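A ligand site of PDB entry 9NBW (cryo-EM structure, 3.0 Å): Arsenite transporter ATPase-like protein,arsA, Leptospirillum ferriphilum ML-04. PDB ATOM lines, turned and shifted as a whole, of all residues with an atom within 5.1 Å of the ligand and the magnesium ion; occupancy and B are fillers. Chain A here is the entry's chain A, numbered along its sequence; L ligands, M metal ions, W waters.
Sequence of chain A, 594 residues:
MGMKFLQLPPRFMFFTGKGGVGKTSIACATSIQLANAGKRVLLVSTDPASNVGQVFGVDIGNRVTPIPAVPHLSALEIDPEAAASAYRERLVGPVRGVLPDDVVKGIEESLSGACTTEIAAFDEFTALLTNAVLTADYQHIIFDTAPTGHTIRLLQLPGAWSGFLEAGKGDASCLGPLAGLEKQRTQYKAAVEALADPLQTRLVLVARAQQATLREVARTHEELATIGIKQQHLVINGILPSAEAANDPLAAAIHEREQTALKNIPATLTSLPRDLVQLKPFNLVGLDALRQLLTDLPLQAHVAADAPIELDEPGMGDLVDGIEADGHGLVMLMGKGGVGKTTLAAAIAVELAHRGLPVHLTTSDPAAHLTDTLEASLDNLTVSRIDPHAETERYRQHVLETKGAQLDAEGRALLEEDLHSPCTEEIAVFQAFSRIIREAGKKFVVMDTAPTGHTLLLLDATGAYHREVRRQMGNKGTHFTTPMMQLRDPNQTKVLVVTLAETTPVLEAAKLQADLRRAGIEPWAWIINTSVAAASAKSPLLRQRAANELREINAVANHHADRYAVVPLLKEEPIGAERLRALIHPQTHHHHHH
The backbone NH (N) of Thr 342 sits close to an oxygen (O5) of the ligand (3.0 Å). The side-chain carboxylate of Glu 573 is in hydrogen-bond range of an oxygen (O13) of the ligand, at 3.0 Å. N of Lys 341 is in hydrogen-bond range of O4 of the ligand, at 3.1 Å. NZ of Lys 341 is in salt-bridge range of O3 of the ligand (3.8 Å). The backbone NH of Val 339 lies within hydrogen-bond range of an oxygen (O4) of the ligand, at 3.3 Å. N of Gly 340 sits at hydrogen-bond distance from O4 of the ligand. A nitrogen (N2) of the ligand is in hydrogen-bond range of the side-chain amide nitrogen of Asn 529 (3.1 Å). The backbone NH (N) of Leu 570 lies within hydrogen-bond range of a nitrogen (N4) of the ligand, at 2.9 Å. An oxygen (O2) of the ligand is in salt-bridge range of the side-chain amino group of Lys 18 (3.5 Å). An oxygen (O2) of the ligand is in hydrogen-bond range of the backbone NH (N) of Gly 19, 3.2 Å away. OG1 of Thr 343 is in hydrogen-bond range of O8 of the ligand (3.0 Å). The backbone carbonyl oxygen of Pro 568 is in hydrogen-bond range of a nitrogen (N3) of the ligand. The backbone NH (N) of Gly 338 is in hydrogen-bond range of an oxygen (O3) of the ligand, at 3.0 Å.
The backbone carbonyl oxygen of Val 339 sits at hydrogen-bond distance from the side-chain amide nitrogen of Asn 529 (3.0 Å). The side-chain carboxylate (OE2) of Glu 573 lies within salt-bridge range of the guanidinium group (NE) of Arg 257. The backbone carbonyl oxygen of Val 567 sits at hydrogen-bond distance from the backbone NH of Thr 530 (3.0 Å). N of Thr 342 lies close to OD2 of Asp 448, 3.3 Å away.
Merely in contact with the magnesium ion: Asp 448 (3.0 Å). Within 4 Å of the magnesium ion: Thr 342 and Asp 448. The nearest printed residue that does not touch the magnesium ion is Asp 365 (4.1 Å).
Water W2 lies within hydrogen-bond range of O of Thr 449 (2.6 Å), OD1 of Asp 448 (2.7 Å) and O1 of the ligand (3.3 Å). Water W1 lies within hydrogen-bond range of O1 of the ligand (2.6 Å), ND1 of His 369 (2.7 Å) and OD2 of Asp 365 (3.1 Å).
The magnesium ion is bound by water W1, water W2, OG1 of Thr 342 and O5 of the ligand. The magnesium ion has four donor atoms within binding distance. Slightly farther from the magnesium ion lies O1 of the ligand (2.8 Å).
The side-chain carboxylate (OD2) of Asp 365 sits close to an oxygen (O1) of the ligand. Gln 210 touches the ligand. Ala 212 touches the ligand. Gly 337 touches the ligand. CG1 of Val 567 touches N3 of the ligand (3.8 Å). Leu 569 touches the ligand. CD of Pro 574 touches C10 of the ligand, 3.9 Å away. Hydrophobic or aromatic side chains within 4 Å of the ligand: Ala 212, Val 567, Leu 569, Leu 570 and Pro 574. Within 4 Å of the ligand: Lys 18, Gly 19, Gln 210, Ala 212, Gly 337, Gly 338, Val 339, Gly 340, Lys 341, Thr 342, Thr 343, Asp 365, Asn 529, Val 567, Pro 568, Leu 569, Leu 570, Glu 573 and Pro 574.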
ATOM      1  N   LYS A  18     -10.701  35.166  19.320  1.00  0.00           N
ATOM      2  CA  LYS A  18     -10.648  35.001  20.766  1.00  0.00           C
ATOM      3  C   LYS A  18      -9.391  35.666  21.323  1.00  0.00           C
ATOM      4  O   LYS A  18      -8.450  35.992  20.602  1.00  0.00           O
ATOM      5  CB  LYS A  18     -10.681  33.518  21.126  1.00  0.00           C
ATOM      6  CG  LYS A  18     -10.996  33.243  22.585  1.00  0.00           C
ATOM      7  CD  LYS A  18     -11.306  31.774  22.819  1.00  0.00           C
ATOM      8  CE  LYS A  18     -10.896  31.338  24.215  1.00  0.00           C
ATOM      9  NZ  LYS A  18      -9.434  31.466  24.431  1.00  0.00           N
ATOM     10  N   GLY A  19      -9.387  35.868  22.640  1.00  0.00           N
ATOM     11  CA  GLY A  19      -8.269  36.556  23.267  1.00  0.00           C
ATOM     12  C   GLY A  19      -6.986  35.754  23.177  1.00  0.00           C
ATOM     13  O   GLY A  19      -6.989  34.520  23.255  1.00  0.00           O
ATOM     14  N   PRO A 147     -10.653  41.044  21.966  1.00  0.00           N
ATOM     15  CA  PRO A 147     -11.227  39.713  21.774  1.00  0.00           C
ATOM     16  C   PRO A 147     -12.663  39.795  21.300  1.00  0.00           C
ATOM     17  O   PRO A 147     -13.387  40.755  21.600  1.00  0.00           O
ATOM     18  CB  PRO A 147     -11.114  39.078  23.162  1.00  0.00           C
ATOM     19  CG  PRO A 147      -9.922  39.731  23.746  1.00  0.00           C
ATOM     20  CD  PRO A 147     -10.013  41.167  23.287  1.00  0.00           C
ATOM     21  N   GLN A 210      -6.517  25.030  18.597  1.00  0.00           N
ATOM     22  CA  GLN A 210      -7.196  24.617  19.816  1.00  0.00           C
ATOM     23  C   GLN A 210      -8.690  24.638  19.526  1.00  0.00           C
ATOM     24  O   GLN A 210      -9.173  25.499  18.784  1.00  0.00           O
ATOM     25  CB  GLN A 210      -6.877  25.514  21.017  1.00  0.00           C
ATOM     26  CG  GLN A 210      -5.404  25.592  21.360  1.00  0.00           C
ATOM     27  CD  GLN A 210      -5.076  26.791  22.226  1.00  0.00           C
ATOM     28  OE1 GLN A 210      -5.945  27.576  22.581  1.00  0.00           O
ATOM     29  NE2 GLN A 210      -3.803  26.933  22.568  1.00  0.00           N
ATOM     30  N   ALA A 212     -11.265  25.315  21.452  1.00  0.00           N
ATOM     31  CA  ALA A 212     -12.007  26.448  21.993  1.00  0.00           C
ATOM     32  C   ALA A 212     -11.896  27.666  21.097  1.00  0.00           C
ATOM     33  O   ALA A 212     -12.900  28.341  20.805  1.00  0.00           O
ATOM     34  CB  ALA A 212     -11.498  26.779  23.397  1.00  0.00           C
ATOM     35  N   ARG A 257      -2.459  17.131  19.668  1.00  0.00           N
ATOM     36  CA  ARG A 257      -3.690  17.853  19.971  1.00  0.00           C
ATOM     37  C   ARG A 257      -3.982  18.912  18.913  1.00  0.00           C
ATOM     38  O   ARG A 257      -5.132  19.070  18.497  1.00  0.00           O
ATOM     39  CB  ARG A 257      -3.586  18.481  21.357  1.00  0.00           C
ATOM     40  CG  ARG A 257      -4.888  19.077  21.849  1.00  0.00           C
ATOM     41  CD  ARG A 257      -4.762  19.582  23.278  1.00  0.00           C
ATOM     42  NE  ARG A 257      -3.926  20.776  23.351  1.00  0.00           N
ATOM     43  CZ  ARG A 257      -2.815  20.893  24.082  1.00  0.00           C
ATOM     44  NH1 ARG A 257      -2.362  19.897  24.821  1.00  0.00           N
ATOM     45  NH2 ARG A 257      -2.151  22.038  24.059  1.00  0.00           N
ATOM     46  N   LYS A 336      -4.856  39.833  31.068  1.00  0.00           N
ATOM     47  CA  LYS A 336      -4.896  39.983  29.623  1.00  0.00           C
ATOM     48  C   LYS A 336      -5.670  38.830  28.984  1.00  0.00           C
ATOM     49  O   LYS A 336      -5.810  37.748  29.556  1.00  0.00           O
ATOM     50  CB  LYS A 336      -3.476  40.046  29.053  1.00  0.00           C
ATOM     51  CG  LYS A 336      -3.395  40.186  27.545  1.00  0.00           C
ATOM     52  CD  LYS A 336      -1.963  40.374  27.087  1.00  0.00           C
ATOM     53  CE  LYS A 336      -1.869  40.484  25.579  1.00  0.00           C
ATOM     54  NZ  LYS A 336      -2.141  39.193  24.913  1.00  0.00           N
ATOM     55  N   GLY A 337      -6.188  39.081  27.786  1.00  0.00           N
ATOM     56  CA  GLY A 337      -6.973  38.073  27.102  1.00  0.00           C
ATOM     57  C   GLY A 337      -6.115  36.868  26.724  1.00  0.00           C
ATOM     58  O   GLY A 337      -4.959  36.999  26.345  1.00  0.00           O
ATOM     59  N   GLY A 338      -6.719  35.682  26.817  1.00  0.00           N
ATOM     60  CA  GLY A 338      -6.064  34.457  26.434  1.00  0.00           C
ATOM     61  C   GLY A 338      -5.038  33.934  27.422  1.00  0.00           C
ATOM     62  O   GLY A 338      -4.307  33.002  27.086  1.00  0.00           O
ATOM     63  N   VAL A 339      -4.984  34.500  28.627  1.00  0.00           N
ATOM     64  CA  VAL A 339      -3.997  34.064  29.615  1.00  0.00           C
ATOM     65  C   VAL A 339      -4.467  32.879  30.444  1.00  0.00           C
ATOM     66  O   VAL A 339      -3.641  32.228  31.095  1.00  0.00           O
ATOM     67  CB  VAL A 339      -3.618  35.227  30.561  1.00  0.00           C
ATOM     68  CG1 VAL A 339      -2.992  36.369  29.773  1.00  0.00           C
ATOM     69  CG2 VAL A 339      -4.825  35.691  31.359  1.00  0.00           C
ATOM     70  N   GLY A 340      -5.772  32.591  30.445  1.00  0.00           N
ATOM     71  CA  GLY A 340      -6.290  31.457  31.189  1.00  0.00           C
ATOM     72  C   GLY A 340      -7.191  31.861  32.334  1.00  0.00           C
ATOM     73  O   GLY A 340      -7.254  31.168  33.351  1.00  0.00           O
ATOM     74  N   LYS A 341      -7.901  32.986  32.180  1.00  0.00           N
ATOM     75  CA  LYS A 341      -8.790  33.440  33.240  1.00  0.00           C
ATOM     76  C   LYS A 341      -9.922  32.453  33.469  1.00  0.00           C
ATOM     77  O   LYS A 341     -10.230  32.089  34.612  1.00  0.00           O
ATOM     78  CB  LYS A 341      -9.351  34.814  32.894  1.00  0.00           C
ATOM     79  CG  LYS A 341      -8.321  35.936  32.964  1.00  0.00           C
ATOM     80  CD  LYS A 341      -8.756  37.188  32.200  1.00  0.00           C
ATOM     81  CE  LYS A 341      -8.883  36.953  30.699  1.00  0.00           C
ATOM     82  NZ  LYS A 341      -9.453  38.136  30.001  1.00  0.00           N
ATOM     83  N   THR A 342     -10.570  32.001  32.392  1.00  0.00           N
ATOM     84  CA  THR A 342     -11.693  31.087  32.527  1.00  0.00           C
ATOM     85  C   THR A 342     -11.254  29.752  33.105  1.00  0.00           C
ATOM     86  O   THR A 342     -11.903  29.203  33.997  1.00  0.00           O
ATOM     87  CB  THR A 342     -12.373  30.869  31.174  1.00  0.00           C
ATOM     88  OG1 THR A 342     -12.682  32.142  30.582  1.00  0.00           O
ATOM     89  CG2 THR A 342     -13.657  30.073  31.334  1.00  0.00           C
ATOM     90  N   THR A 343     -10.141  29.201  32.603  1.00  0.00           N
ATOM     91  CA  THR A 343      -9.670  27.920  33.083  1.00  0.00           C
ATOM     92  C   THR A 343      -9.330  27.978  34.570  1.00  0.00           C
ATOM     93  O   THR A 343      -9.714  27.090  35.343  1.00  0.00           O
ATOM     94  CB  THR A 343      -8.443  27.486  32.275  1.00  0.00           C
ATOM     95  OG1 THR A 343      -8.851  27.098  30.954  1.00  0.00           O
ATOM     96  CG2 THR A 343      -7.739  26.309  32.939  1.00  0.00           C
ATOM     97  N   ASP A 365     -17.694  37.908  30.965  1.00  0.00           N
ATOM     98  CA  ASP A 365     -17.315  37.952  29.555  1.00  0.00           C
ATOM     99  C   ASP A 365     -18.553  37.793  28.692  1.00  0.00           C
ATOM    100  O   ASP A 365     -19.321  36.841  28.882  1.00  0.00           O
ATOM    101  CB  ASP A 365     -16.303  36.847  29.265  1.00  0.00           C
ATOM    102  CG  ASP A 365     -15.654  36.991  27.901  1.00  0.00           C
ATOM    103  OD1 ASP A 365     -15.997  37.923  27.159  1.00  0.00           O
ATOM    104  OD2 ASP A 365     -14.793  36.151  27.576  1.00  0.00           O
ATOM    105  N   HIS A 369     -17.398  31.016  28.417  1.00  0.00           N
ATOM    106  CA  HIS A 369     -16.840  29.698  28.153  1.00  0.00           C
ATOM    107  C   HIS A 369     -16.785  28.855  29.418  1.00  0.00           C
ATOM    108  O   HIS A 369     -15.826  28.128  29.639  1.00  0.00           O
ATOM    109  CB  HIS A 369     -15.445  29.813  27.538  1.00  0.00           C
ATOM    110  CG  HIS A 369     -15.343  30.841  26.453  1.00  0.00           C
ATOM    111  ND1 HIS A 369     -14.423  31.870  26.476  1.00  0.00           N
ATOM    112  CD2 HIS A 369     -16.054  31.010  25.308  1.00  0.00           C
ATOM    113  CE1 HIS A 369     -14.563  32.617  25.401  1.00  0.00           C
ATOM    114  NE2 HIS A 369     -15.542  32.118  24.677  1.00  0.00           N
ATOM    115  N   ASP A 448     -14.907  35.047  36.829  1.00  0.00           N
ATOM    116  CA  ASP A 448     -14.090  35.266  35.652  1.00  0.00           C
ATOM    117  C   ASP A 448     -14.529  36.555  34.968  1.00  0.00           C
ATOM    118  O   ASP A 448     -15.719  36.818  34.816  1.00  0.00           O
ATOM    119  CB  ASP A 448     -14.229  34.084  34.687  1.00  0.00           C
ATOM    120  CG  ASP A 448     -13.396  34.251  33.441  1.00  0.00           C
ATOM    121  OD1 ASP A 448     -12.578  35.188  33.376  1.00  0.00           O
ATOM    122  OD2 ASP A 448     -13.568  33.437  32.506  1.00  0.00           O
ATOM    123  N   THR A 449     -13.557  37.353  34.547  1.00  0.00           N
ATOM    124  CA  THR A 449     -13.829  38.660  33.964  1.00  0.00           C
ATOM    125  C   THR A 449     -13.498  38.646  32.471  1.00  0.00           C
ATOM    126  O   THR A 449     -12.992  37.665  31.920  1.00  0.00           O
ATOM    127  CB  THR A 449     -13.028  39.742  34.678  1.00  0.00           C
ATOM    128  OG1 THR A 449     -11.643  39.637  34.335  1.00  0.00           O
ATOM    129  CG2 THR A 449     -13.189  39.625  36.180  1.00  0.00           C
ATOM    130  N   PRO A 451     -11.450  40.803  29.227  1.00  0.00           N
ATOM    131  CA  PRO A 451     -10.105  41.397  29.154  1.00  0.00           C
ATOM    132  C   PRO A 451     -10.016  42.671  29.963  1.00  0.00           C
ATOM    133  O   PRO A 451     -11.014  43.247  30.406  1.00  0.00           O
ATOM    134  CB  PRO A 451      -9.911  41.641  27.664  1.00  0.00           C
ATOM    135  CG  PRO A 451     -10.740  40.599  27.012  1.00  0.00           C
ATOM    136  CD  PRO A 451     -11.954  40.447  27.886  1.00  0.00           C
ATOM    137  N   ASN A 529       0.304  31.523  34.175  1.00  0.00           N
ATOM    138  CA  ASN A 529      -0.347  30.357  33.613  1.00  0.00           C
ATOM    139  C   ASN A 529       0.241  29.899  32.284  1.00  0.00           C
ATOM    140  O   ASN A 529       0.683  30.708  31.466  1.00  0.00           O
ATOM    141  CB  ASN A 529      -1.806  30.662  33.300  1.00  0.00           C
ATOM    142  CG  ASN A 529      -2.651  29.412  33.180  1.00  0.00           C
ATOM    143  OD1 ASN A 529      -2.468  28.444  33.919  1.00  0.00           O
ATOM    144  ND2 ASN A 529      -3.584  29.418  32.236  1.00  0.00           N
ATOM    145  N   THR A 530       0.244  28.583  32.089  1.00  0.00           N
ATOM    146  CA  THR A 530       0.700  27.943  30.862  1.00  0.00           C
ATOM    147  C   THR A 530       2.119  28.414  30.546  1.00  0.00           C
ATOM    148  O   THR A 530       2.419  28.931  29.470  1.00  0.00           O
ATOM    149  CB  THR A 530      -0.235  28.158  29.659  1.00  0.00           C
ATOM    150  OG1 THR A 530       0.289  27.483  28.506  1.00  0.00           O
ATOM    151  CG2 THR A 530      -0.429  29.634  29.342  1.00  0.00           C
ATOM    152  N   VAL A 567       1.517  27.841  36.989  1.00  0.00           N
ATOM    153  CA  VAL A 567       0.789  26.703  36.435  1.00  0.00           C
ATOM    154  C   VAL A 567       1.500  26.280  35.148  1.00  0.00           C
ATOM    155  O   VAL A 567       1.644  27.092  34.237  1.00  0.00           O
ATOM    156  CB  VAL A 567      -0.680  27.059  36.158  1.00  0.00           C
ATOM    157  CG1 VAL A 567      -1.426  25.839  35.616  1.00  0.00           C
ATOM    158  CG2 VAL A 567      -1.351  27.580  37.413  1.00  0.00           C
ATOM    159  N   PRO A 568       1.965  25.028  35.045  1.00  0.00           N
ATOM    160  CA  PRO A 568       2.701  24.628  33.837  1.00  0.00           C
ATOM    161  C   PRO A 568       1.815  24.504  32.605  1.00  0.00           C
ATOM    162  O   PRO A 568       0.600  24.690  32.690  1.00  0.00           O
ATOM    163  CB  PRO A 568       3.301  23.270  34.223  1.00  0.00           C
ATOM    164  CG  PRO A 568       2.378  22.744  35.263  1.00  0.00           C
ATOM    165  CD  PRO A 568       1.895  23.931  36.032  1.00  0.00           C
ATOM    166  N   LEU A 569       2.427  24.207  31.465  1.00  0.00           N
ATOM    167  CA  LEU A 569       1.708  24.024  30.201  1.00  0.00           C
ATOM    168  C   LEU A 569       1.275  22.567  30.117  1.00  0.00           C
ATOM    169  O   LEU A 569       2.025  21.700  29.659  1.00  0.00           O
ATOM    170  CB  LEU A 569       2.570  24.431  29.018  1.00  0.00           C
ATOM    171  CG  LEU A 569       2.080  24.050  27.613  1.00  0.00           C
ATOM    172  CD1 LEU A 569       0.902  24.902  27.209  1.00  0.00           C
ATOM    173  CD2 LEU A 569       3.204  24.181  26.614  1.00  0.00           C
ATOM    174  N   LEU A 570       0.063  22.293  30.580  1.00  0.00           N
ATOM    175  CA  LEU A 570      -0.462  20.927  30.553  1.00  0.00           C
ATOM    176  C   LEU A 570      -0.488  20.390  29.136  1.00  0.00           C
ATOM    177  O   LEU A 570      -0.844  21.100  28.188  1.00  0.00           O
ATOM    178  CB  LEU A 570      -1.869  20.893  31.156  1.00  0.00           C
ATOM    179  CG  LEU A 570      -2.038  21.545  32.528  1.00  0.00           C
ATOM    180  CD1 LEU A 570      -3.454  21.337  33.021  1.00  0.00           C
ATOM    181  CD2 LEU A 570      -1.033  20.978  33.523  1.00  0.00           C
ATOM    182  N   GLU A 572      -2.523  18.244  28.099  1.00  0.00           N
ATOM    183  CA  GLU A 572      -3.919  18.056  27.734  1.00  0.00           C
ATOM    184  C   GLU A 572      -4.707  19.230  28.286  1.00  0.00           C
ATOM    185  O   GLU A 572      -4.610  19.548  29.475  1.00  0.00           O
ATOM    186  CB  GLU A 572      -4.470  16.739  28.292  1.00  0.00           C
ATOM    187  CG  GLU A 572      -4.010  15.492  27.536  1.00  0.00           C
ATOM    188  CD  GLU A 572      -4.495  15.476  26.098  1.00  0.00           C
ATOM    189  OE1 GLU A 572      -5.723  15.477  25.886  1.00  0.00           O
ATOM    190  OE2 GLU A 572      -3.640  15.448  25.185  1.00  0.00           O
ATOM    191  N   GLU A 573      -5.496  19.866  27.430  1.00  0.00           N
ATOM    192  CA  GLU A 573      -6.214  21.065  27.839  1.00  0.00           C
ATOM    193  C   GLU A 573      -7.093  20.756  29.043  1.00  0.00           C
ATOM    194  O   GLU A 573      -7.833  19.753  29.029  1.00  0.00           O
ATOM    195  CB  GLU A 573      -7.070  21.607  26.702  1.00  0.00           C
ATOM    196  CG  GLU A 573      -6.274  22.115  25.512  1.00  0.00           C
ATOM    197  CD  GLU A 573      -7.133  22.868  24.520  1.00  0.00           C
ATOM    198  OE1 GLU A 573      -8.329  23.105  24.806  1.00  0.00           O
ATOM    199  OE2 GLU A 573      -6.613  23.229  23.436  1.00  0.00           O
ATOM    200  N   PRO A 574      -7.054  21.554  30.108  1.00  0.00           N
ATOM    201  CA  PRO A 574      -7.869  21.257  31.284  1.00  0.00           C
ATOM    202  C   PRO A 574      -9.343  21.492  31.039  1.00  0.00           C
ATOM    203  O   PRO A 574      -9.805  22.641  30.996  1.00  0.00           O
ATOM    204  CB  PRO A 574      -7.310  22.197  32.358  1.00  0.00           C
ATOM    205  CG  PRO A 574      -6.785  23.345  31.576  1.00  0.00           C
ATOM    206  CD  PRO A 574      -6.234  22.768  30.309  1.00  0.00           C
HETATM  207  P1  LIG L   1     -10.532  35.049  26.693  1.00  0.00           P
HETATM  208  O1  LIG L   1     -11.796  35.226  27.452  1.00  0.00           O
HETATM  209  O2  LIG L   1     -10.744  34.626  25.246  1.00  0.00           O
HETATM  210  O3  LIG L   1      -9.629  36.284  26.734  1.00  0.00           O
HETATM  211  P2  LIG L   1      -9.192  33.356  28.761  1.00  0.00           P
HETATM  212  O4  LIG L   1      -8.152  34.210  29.343  1.00  0.00           O
HETATM  213  O5  LIG L   1     -10.465  33.184  29.587  1.00  0.00           O
HETATM  214  O6  LIG L   1      -9.661  33.883  27.336  1.00  0.00           O
HETATM  215  P3  LIG L   1      -9.256  30.428  28.347  1.00  0.00           P
HETATM  216  O7  LIG L   1     -10.728  30.436  28.422  1.00  0.00           O
HETATM  217  O8  LIG L   1      -8.557  29.616  29.431  1.00  0.00           O
HETATM  218  O9  LIG L   1      -8.656  31.896  28.410  1.00  0.00           O
HETATM  219  O10 LIG L   1      -8.773  29.904  26.944  1.00  0.00           O
HETATM  220  C1  LIG L   1      -7.374  29.889  26.579  1.00  0.00           C
HETATM  221  C2  LIG L   1      -6.920  28.467  26.334  1.00  0.00           C
HETATM  222  O11 LIG L   1      -5.825  28.248  27.228  1.00  0.00           O
HETATM  223  C3  LIG L   1      -7.952  27.451  26.813  1.00  0.00           C
HETATM  224  O12 LIG L   1      -8.587  26.966  25.637  1.00  0.00           O
HETATM  225  C4  LIG L   1      -7.095  26.295  27.355  1.00  0.00           C
HETATM  226  O13 LIG L   1      -7.089  25.302  26.338  1.00  0.00           O
HETATM  227  C5  LIG L   1      -5.675  26.858  27.337  1.00  0.00           C
HETATM  228  N1  LIG L   1      -4.991  26.618  28.601  1.00  0.00           N
HETATM  229  C6  LIG L   1      -5.196  27.287  29.790  1.00  0.00           C
HETATM  230  N2  LIG L   1      -4.446  26.867  30.766  1.00  0.00           N
HETATM  231  C7  LIG L   1      -3.680  25.859  30.202  1.00  0.00           C
HETATM  232  C8  LIG L   1      -2.685  25.011  30.710  1.00  0.00           C
HETATM  233  N3  LIG L   1      -2.256  25.042  31.977  1.00  0.00           N
HETATM  234  N4  LIG L   1      -2.125  24.109  29.868  1.00  0.00           N
HETATM  235  C9  LIG L   1      -2.547  24.071  28.602  1.00  0.00           C
HETATM  236  N5  LIG L   1      -3.471  24.819  28.007  1.00  0.00           N
HETATM  237  C10 LIG L   1      -4.014  25.697  28.862  1.00  0.00           C
HETATM  238 MG    MG M   1     -12.255  33.784  29.804  1.00  0.00          MG
HETATM  239  O   HOH W   1     -13.433  33.463  28.470  1.00  0.00           O
HETATM  240  O   HOH W   2     -12.633  35.354  30.681  1.00  0.00           O
HETATM  241  O   HOH W   3     -13.476  36.064  23.900  1.00  0.00           O
